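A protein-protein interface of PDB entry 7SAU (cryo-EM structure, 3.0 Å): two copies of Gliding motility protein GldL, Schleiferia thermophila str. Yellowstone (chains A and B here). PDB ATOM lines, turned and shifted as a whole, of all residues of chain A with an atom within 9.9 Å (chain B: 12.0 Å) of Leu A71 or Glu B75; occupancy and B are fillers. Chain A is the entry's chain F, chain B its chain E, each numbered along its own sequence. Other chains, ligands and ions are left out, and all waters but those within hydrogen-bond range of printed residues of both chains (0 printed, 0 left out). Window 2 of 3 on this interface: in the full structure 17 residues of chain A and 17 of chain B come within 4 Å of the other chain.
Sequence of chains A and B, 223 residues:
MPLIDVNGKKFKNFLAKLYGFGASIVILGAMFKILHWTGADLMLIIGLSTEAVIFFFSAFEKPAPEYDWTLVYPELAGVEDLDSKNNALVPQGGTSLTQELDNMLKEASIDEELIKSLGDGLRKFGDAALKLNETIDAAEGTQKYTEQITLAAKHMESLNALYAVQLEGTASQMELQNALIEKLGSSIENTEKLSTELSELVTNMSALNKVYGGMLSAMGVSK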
ATOM      1  N   GLU A  66      18.161  14.337  -7.502  1.00  0.00           N
ATOM      2  CA  GLU A  66      16.932  14.313  -6.708  1.00  0.00           C
ATOM      3  C   GLU A  66      17.057  13.337  -5.536  1.00  0.00           C
ATOM      4  O   GLU A  66      16.358  12.327  -5.448  1.00  0.00           O
ATOM      5  CB  GLU A  66      15.723  13.974  -7.588  1.00  0.00           C
ATOM      6  CG  GLU A  66      14.376  14.295  -6.960  1.00  0.00           C
ATOM      7  CD  GLU A  66      13.989  15.750  -7.122  1.00  0.00           C
ATOM      8  OE1 GLU A  66      14.389  16.366  -8.132  1.00  0.00           O
ATOM      9  OE2 GLU A  66      13.282  16.280  -6.240  1.00  0.00           O
ATOM     10  N   TYR A  67      17.979  13.660  -4.636  1.00  0.00           N
ATOM     11  CA  TYR A  67      18.276  12.781  -3.513  1.00  0.00           C
ATOM     12  C   TYR A  67      17.131  12.764  -2.511  1.00  0.00           C
ATOM     13  O   TYR A  67      16.494  13.786  -2.248  1.00  0.00           O
ATOM     14  CB  TYR A  67      19.566  13.223  -2.831  1.00  0.00           C
ATOM     15  CG  TYR A  67      20.803  12.856  -3.608  1.00  0.00           C
ATOM     16  CD1 TYR A  67      20.765  11.857  -4.568  1.00  0.00           C
ATOM     17  CD2 TYR A  67      21.999  13.523  -3.405  1.00  0.00           C
ATOM     18  CE1 TYR A  67      21.888  11.518  -5.286  1.00  0.00           C
ATOM     19  CE2 TYR A  67      23.126  13.196  -4.124  1.00  0.00           C
ATOM     20  CZ  TYR A  67      23.066  12.191  -5.062  1.00  0.00           C
ATOM     21  OH  TYR A  67      24.188  11.857  -5.782  1.00  0.00           O
ATOM     22  N   ASP A  68      16.875  11.587  -1.950  1.00  0.00           N
ATOM     23  CA  ASP A  68      15.889  11.403  -0.897  1.00  0.00           C
ATOM     24  C   ASP A  68      16.609  11.156   0.420  1.00  0.00           C
ATOM     25  O   ASP A  68      17.566  10.378   0.479  1.00  0.00           O
ATOM     26  CB  ASP A  68      14.954  10.235  -1.215  1.00  0.00           C
ATOM     27  CG  ASP A  68      13.771  10.159  -0.273  1.00  0.00           C
ATOM     28  OD1 ASP A  68      13.666  11.016   0.631  1.00  0.00           O
ATOM     29  OD2 ASP A  68      12.941   9.241  -0.437  1.00  0.00           O
ATOM     30  N   TRP A  69      16.155  11.833   1.475  1.00  0.00           N
ATOM     31  CA  TRP A  69      16.803  11.747   2.774  1.00  0.00           C
ATOM     32  C   TRP A  69      15.956  11.075   3.841  1.00  0.00           C
ATOM     33  O   TRP A  69      16.497  10.698   4.884  1.00  0.00           O
ATOM     34  CB  TRP A  69      17.201  13.147   3.262  1.00  0.00           C
ATOM     35  CG  TRP A  69      18.237  13.798   2.402  1.00  0.00           C
ATOM     36  CD1 TRP A  69      18.025  14.707   1.410  1.00  0.00           C
ATOM     37  CD2 TRP A  69      19.651  13.586   2.453  1.00  0.00           C
ATOM     38  NE1 TRP A  69      19.216  15.075   0.841  1.00  0.00           N
ATOM     39  CE2 TRP A  69      20.231  14.400   1.464  1.00  0.00           C
ATOM     40  CE3 TRP A  69      20.482  12.787   3.240  1.00  0.00           C
ATOM     41  CZ2 TRP A  69      21.602  14.439   1.242  1.00  0.00           C
ATOM     42  CZ3 TRP A  69      21.843  12.827   3.017  1.00  0.00           C
ATOM     43  CH2 TRP A  69      22.389  13.647   2.028  1.00  0.00           C
ATOM     44  N   THR A  70      14.651  10.917   3.612  1.00  0.00           N
ATOM     45  CA  THR A  70      13.796  10.291   4.615  1.00  0.00           C
ATOM     46  C   THR A  70      14.177   8.836   4.844  1.00  0.00           C
ATOM     47  O   THR A  70      14.154   8.353   5.981  1.00  0.00           O
ATOM     48  CB  THR A  70      12.330  10.395   4.198  1.00  0.00           C
ATOM     49  OG1 THR A  70      12.140   9.721   2.948  1.00  0.00           O
ATOM     50  CG2 THR A  70      11.918  11.848   4.055  1.00  0.00           C
ATOM     51  N   LEU A  71      14.526   8.116   3.776  1.00  0.00           N
ATOM     52  CA  LEU A  71      14.810   6.691   3.912  1.00  0.00           C
ATOM     53  C   LEU A  71      16.081   6.448   4.716  1.00  0.00           C
ATOM     54  O   LEU A  71      16.274   5.360   5.272  1.00  0.00           O
ATOM     55  CB  LEU A  71      14.907   6.026   2.537  1.00  0.00           C
ATOM     56  CG  LEU A  71      16.128   6.270   1.650  1.00  0.00           C
ATOM     57  CD1 LEU A  71      16.173   5.229   0.549  1.00  0.00           C
ATOM     58  CD2 LEU A  71      16.096   7.653   1.047  1.00  0.00           C
ATOM     59  N   VAL A  72      16.964   7.446   4.790  1.00  0.00           N
ATOM     60  CA  VAL A  72      18.161   7.340   5.619  1.00  0.00           C
ATOM     61  C   VAL A  72      18.083   8.197   6.874  1.00  0.00           C
ATOM     62  O   VAL A  72      18.921   8.030   7.775  1.00  0.00           O
ATOM     63  CB  VAL A  72      19.433   7.694   4.820  1.00  0.00           C
ATOM     64  CG1 VAL A  72      19.644   6.684   3.707  1.00  0.00           C
ATOM     65  CG2 VAL A  72      19.328   9.094   4.254  1.00  0.00           C
ATOM     66  N   TYR A  73      17.116   9.111   6.961  1.00  0.00           N
ATOM     67  CA  TYR A  73      16.827   9.873   8.175  1.00  0.00           C
ATOM     68  C   TYR A  73      15.328   9.755   8.421  1.00  0.00           C
ATOM     69  O   TYR A  73      14.551  10.632   8.015  1.00  0.00           O
ATOM     70  CB  TYR A  73      17.258  11.333   8.053  1.00  0.00           C
ATOM     71  CG  TYR A  73      18.754  11.553   8.090  1.00  0.00           C
ATOM     72  CD1 TYR A  73      19.345  12.227   9.144  1.00  0.00           C
ATOM     73  CD2 TYR A  73      19.569  11.115   7.058  1.00  0.00           C
ATOM     74  CE1 TYR A  73      20.708  12.439   9.183  1.00  0.00           C
ATOM     75  CE2 TYR A  73      20.932  11.322   7.087  1.00  0.00           C
ATOM     76  CZ  TYR A  73      21.496  11.986   8.151  1.00  0.00           C
ATOM     77  OH  TYR A  73      22.854  12.198   8.186  1.00  0.00           O
ATOM     78  N   PRO A  74      14.885   8.677   9.076  1.00  0.00           N
ATOM     79  CA  PRO A  74      13.446   8.380   9.146  1.00  0.00           C
ATOM     80  C   PRO A  74      12.611   9.491   9.764  1.00  0.00           C
ATOM     81  O   PRO A  74      13.031  10.142  10.726  1.00  0.00           O
ATOM     82  CB  PRO A  74      13.396   7.111  10.007  1.00  0.00           C
ATOM     83  CG  PRO A  74      14.737   6.484   9.834  1.00  0.00           C
ATOM     84  CD  PRO A  74      15.702   7.621   9.697  1.00  0.00           C
ATOM     85  N   GLU A  75      11.421   9.700   9.204  1.00  0.00           N
ATOM     86  CA  GLU A  75      10.481  10.724   9.655  1.00  0.00           C
ATOM     87  C   GLU A  75      11.158  12.089   9.732  1.00  0.00           C
ATOM     88  O   GLU A  75      11.342  12.672  10.804  1.00  0.00           O
ATOM     89  CB  GLU A  75       9.851  10.339  10.993  1.00  0.00           C
ATOM     90  CG  GLU A  75       8.635  11.176  11.371  1.00  0.00           C
ATOM     91  CD  GLU A  75       7.702  11.413  10.199  1.00  0.00           C
ATOM     92  OE1 GLU A  75       7.033  10.452   9.765  1.00  0.00           O
ATOM     93  OE2 GLU A  75       7.638  12.561   9.710  1.00  0.00           O
ATOM     94  N   LEU A  76      11.552  12.593   8.569  1.00  0.00           N
ATOM     95  CA  LEU A  76      12.191  13.896   8.489  1.00  0.00           C
ATOM     96  C   LEU A  76      11.180  14.914   7.972  1.00  0.00           C
ATOM     97  O   LEU A  76      11.168  16.066   8.399  1.00  0.00           O
ATOM     98  CB  LEU A  76      13.423  13.838   7.583  1.00  0.00           C
ATOM     99  CG  LEU A  76      14.419  15.001   7.622  1.00  0.00           C
ATOM    100  CD1 LEU A  76      15.781  14.521   7.166  1.00  0.00           C
ATOM    101  CD2 LEU A  76      13.969  16.175   6.779  1.00  0.00           C
ATOM    102  N   ASP B  68      28.040  14.164  -4.924  1.00  0.00           N
ATOM    103  CA  ASP B  68      27.298  12.929  -5.169  1.00  0.00           C
ATOM    104  C   ASP B  68      27.201  12.205  -3.829  1.00  0.00           C
ATOM    105  O   ASP B  68      28.098  11.456  -3.442  1.00  0.00           O
ATOM    106  CB  ASP B  68      27.977  12.075  -6.233  1.00  0.00           C
ATOM    107  CG  ASP B  68      27.155  10.861  -6.614  1.00  0.00           C
ATOM    108  OD1 ASP B  68      26.143  11.029  -7.325  1.00  0.00           O
ATOM    109  OD2 ASP B  68      27.516   9.740  -6.204  1.00  0.00           O
ATOM    110  N   TRP B  69      26.091  12.434  -3.124  1.00  0.00           N
ATOM    111  CA  TRP B  69      25.961  11.990  -1.742  1.00  0.00           C
ATOM    112  C   TRP B  69      25.901  10.475  -1.606  1.00  0.00           C
ATOM    113  O   TRP B  69      26.036   9.963  -0.490  1.00  0.00           O
ATOM    114  CB  TRP B  69      24.713  12.614  -1.121  1.00  0.00           C
ATOM    115  CG  TRP B  69      24.874  14.065  -0.809  1.00  0.00           C
ATOM    116  CD1 TRP B  69      24.327  15.112  -1.488  1.00  0.00           C
ATOM    117  CD2 TRP B  69      25.625  14.634   0.267  1.00  0.00           C
ATOM    118  NE1 TRP B  69      24.696  16.298  -0.906  1.00  0.00           N
ATOM    119  CE2 TRP B  69      25.492  16.030   0.175  1.00  0.00           C
ATOM    120  CE3 TRP B  69      26.396  14.097   1.297  1.00  0.00           C
ATOM    121  CZ2 TRP B  69      26.103  16.895   1.074  1.00  0.00           C
ATOM    122  CZ3 TRP B  69      27.000  14.956   2.187  1.00  0.00           C
ATOM    123  CH2 TRP B  69      26.852  16.339   2.071  1.00  0.00           C
ATOM    124  N   THR B  70      25.697   9.747  -2.706  1.00  0.00           N
ATOM    125  CA  THR B  70      25.561   8.297  -2.614  1.00  0.00           C
ATOM    126  C   THR B  70      26.845   7.631  -2.136  1.00  0.00           C
ATOM    127  O   THR B  70      26.793   6.535  -1.569  1.00  0.00           O
ATOM    128  CB  THR B  70      25.140   7.719  -3.963  1.00  0.00           C
ATOM    129  OG1 THR B  70      26.068   8.136  -4.971  1.00  0.00           O
ATOM    130  CG2 THR B  70      23.747   8.194  -4.332  1.00  0.00           C
ATOM    131  N   LEU B  71      27.999   8.264  -2.358  1.00  0.00           N
ATOM    132  CA  LEU B  71      29.256   7.698  -1.878  1.00  0.00           C
ATOM    133  C   LEU B  71      29.279   7.616  -0.357  1.00  0.00           C
ATOM    134  O   LEU B  71      29.723   6.616   0.217  1.00  0.00           O
ATOM    135  CB  LEU B  71      30.439   8.523  -2.385  1.00  0.00           C
ATOM    136  CG  LEU B  71      31.020   8.170  -3.756  1.00  0.00           C
ATOM    137  CD1 LEU B  71      30.078   8.552  -4.877  1.00  0.00           C
ATOM    138  CD2 LEU B  71      32.373   8.838  -3.944  1.00  0.00           C
ATOM    139  N   VAL B  72      28.799   8.665   0.314  1.00  0.00           N
ATOM    140  CA  VAL B  72      28.808   8.716   1.770  1.00  0.00           C
ATOM    141  C   VAL B  72      27.479   8.276   2.371  1.00  0.00           C
ATOM    142  O   VAL B  72      27.393   8.065   3.587  1.00  0.00           O
ATOM    143  CB  VAL B  72      29.189  10.132   2.252  1.00  0.00           C
ATOM    144  CG1 VAL B  72      28.061  11.105   1.985  1.00  0.00           C
ATOM    145  CG2 VAL B  72      29.596  10.132   3.722  1.00  0.00           C
ATOM    146  N   TYR B  73      26.444   8.103   1.549  1.00  0.00           N
ATOM    147  CA  TYR B  73      25.142   7.626   2.018  1.00  0.00           C
ATOM    148  C   TYR B  73      24.558   6.691   0.970  1.00  0.00           C
ATOM    149  O   TYR B  73      23.801   7.112   0.087  1.00  0.00           O
ATOM    150  CB  TYR B  73      24.200   8.796   2.296  1.00  0.00           C
ATOM    151  CG  TYR B  73      24.386   9.437   3.649  1.00  0.00           C
ATOM    152  CD1 TYR B  73      23.805   8.893   4.783  1.00  0.00           C
ATOM    153  CD2 TYR B  73      25.134  10.596   3.789  1.00  0.00           C
ATOM    154  CE1 TYR B  73      23.971   9.480   6.020  1.00  0.00           C
ATOM    155  CE2 TYR B  73      25.305  11.190   5.021  1.00  0.00           C
ATOM    156  CZ  TYR B  73      24.721  10.628   6.133  1.00  0.00           C
ATOM    157  OH  TYR B  73      24.890  11.218   7.364  1.00  0.00           O
ATOM    158  N   PRO B  74      24.914   5.410   1.020  1.00  0.00           N
ATOM    159  CA  PRO B  74      24.345   4.448   0.068  1.00  0.00           C
ATOM    160  C   PRO B  74      22.825   4.443   0.131  1.00  0.00           C
ATOM    161  O   PRO B  74      22.230   4.504   1.210  1.00  0.00           O
ATOM    162  CB  PRO B  74      24.928   3.103   0.518  1.00  0.00           C
ATOM    163  CG  PRO B  74      25.996   3.405   1.515  1.00  0.00           C
ATOM    164  CD  PRO B  74      26.080   4.875   1.742  1.00  0.00           C
ATOM    165  N   GLU B  75      22.200   4.366  -1.043  1.00  0.00           N
ATOM    166  CA  GLU B  75      20.745   4.412  -1.175  1.00  0.00           C
ATOM    167  C   GLU B  75      20.182   5.666  -0.508  1.00  0.00           C
ATOM    168  O   GLU B  75      19.428   5.605   0.465  1.00  0.00           O
ATOM    169  CB  GLU B  75      20.102   3.142  -0.611  1.00  0.00           C
ATOM    170  CG  GLU B  75      18.630   2.962  -0.963  1.00  0.00           C
ATOM    171  CD  GLU B  75      18.397   2.778  -2.451  1.00  0.00           C
ATOM    172  OE1 GLU B  75      19.313   2.288  -3.145  1.00  0.00           O
ATOM    173  OE2 GLU B  75      17.296   3.125  -2.927  1.00  0.00           O
ATOM    174  N   LEU B  76      20.578   6.821  -1.035  1.00  0.00           N
ATOM    175  CA  LEU B  76      20.136   8.105  -0.504  1.00  0.00           C
ATOM    176  C   LEU B  76      20.321   9.217  -1.524  1.00  0.00           C
ATOM    177  O   LEU B  76      20.980  10.218  -1.245  1.00  0.00           O
ATOM    178  CB  LEU B  76      20.895   8.451   0.777  1.00  0.00           C
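OD2 of Asp B68 lies within hydrogen-bond range of OG1 of Thr B70, at 2.5 Å.
The side-chain carboxylate (OD1) of Asp A68 sits at hydrogen-bond distance from the side-chain hydroxyl (OG1) of Thr A70.
Of the 11 printed residues of chain A, 6 touch a printed residue of chain B.
Among the printed residues, 10 pairs touch across the chains.
Among the printed residues, no Asp or Glu carboxylate lies within 4 Å of a Lys or Arg side-chain nitrogen of the other chain.
Of chain B, only Glu B75 comes within 4 Å of Leu A71.
Of chain A, only Leu A71 (3.3 Å) and Val A72 (3.4 Å) come within 4 Å of Glu B75.
Of chain B, only Leu B76 (3.6 Å) comes within 4 Å of Asp A68.
No residue of chain B comes within 4 Å of Thr A70.
Of the printed residues of chain B, Val A72 touches Glu B75 (3.4 Å) and Leu B76 (3.6 Å).
Pro A74 touches none of the printed residues of chain B.
Of chain A, only Tyr A67 (3.5 Å), Asp A68 (3.6 Å) and Val A72 (3.6 Å) come within 4 Å of Leu B76.
Of the printed residues of chain A, Tyr B73 touches Tyr A73.
Printed residues of chain B within 4 Å of Tyr A73: Tyr B73.
Of the printed residues of chain A, Asp B68 touches Tyr A67.
Glu A66 touches none of the printed residues of chain B.
Val B72 touches none of the printed residues of chain A.
The nearest residue of chain B that does not touch Leu A71 is Leu B76 (4.4 Å).
The nearest residue of chain A that does not touch Glu B75 is Asp A68 (5.1 Å).
The nearest printed residue of chain B that does not touch Trp A69 is Tyr B73 (4.1 Å).
Asp A68 touches Leu B76, but with the chains exchanged Leu A76 does not touch Asp B68 (16.0 Å).
Trp B69 touches its own counterpart, Trp A69.
Leu A71 touches Glu B75, but with the chains exchanged Glu A75 does not touch Leu B71 (20.3 Å).
Val A72 touches Glu B75, but with the chains exchanged Glu A75 does not touch Val B72 (17.0 Å).
9 positions are printed for both chains.
Of the 10 pairs that touch across the chains among the printed residues, 2 have their exchanged pair printed and touching as well.
OD1 of Asp B68 lies within hydrogen-bond range of OH of Tyr A67.
The side-chain hydroxyl (OH) of Tyr A67 lies close to the backbone NH (N) of Trp B69, at 3.3 Å.
OH of Tyr B73 is in hydrogen-bond range of OH of Tyr A73, at 2.4 Å.
Among the printed residues, pairs that only touch across the chains: Tyr A67 with Thr B70 (3.9 Å), Tyr A67 with Leu B76 (3.5 Å), Asp A68 with Leu B76 (3.6 Å), Trp A69 with Trp B69 (3.8 Å), Leu A71 with Glu B75 (3.3 Å), Val A72 with Glu B75 (3.4 Å) and Val A72 with Leu B76 (3.6 Å).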
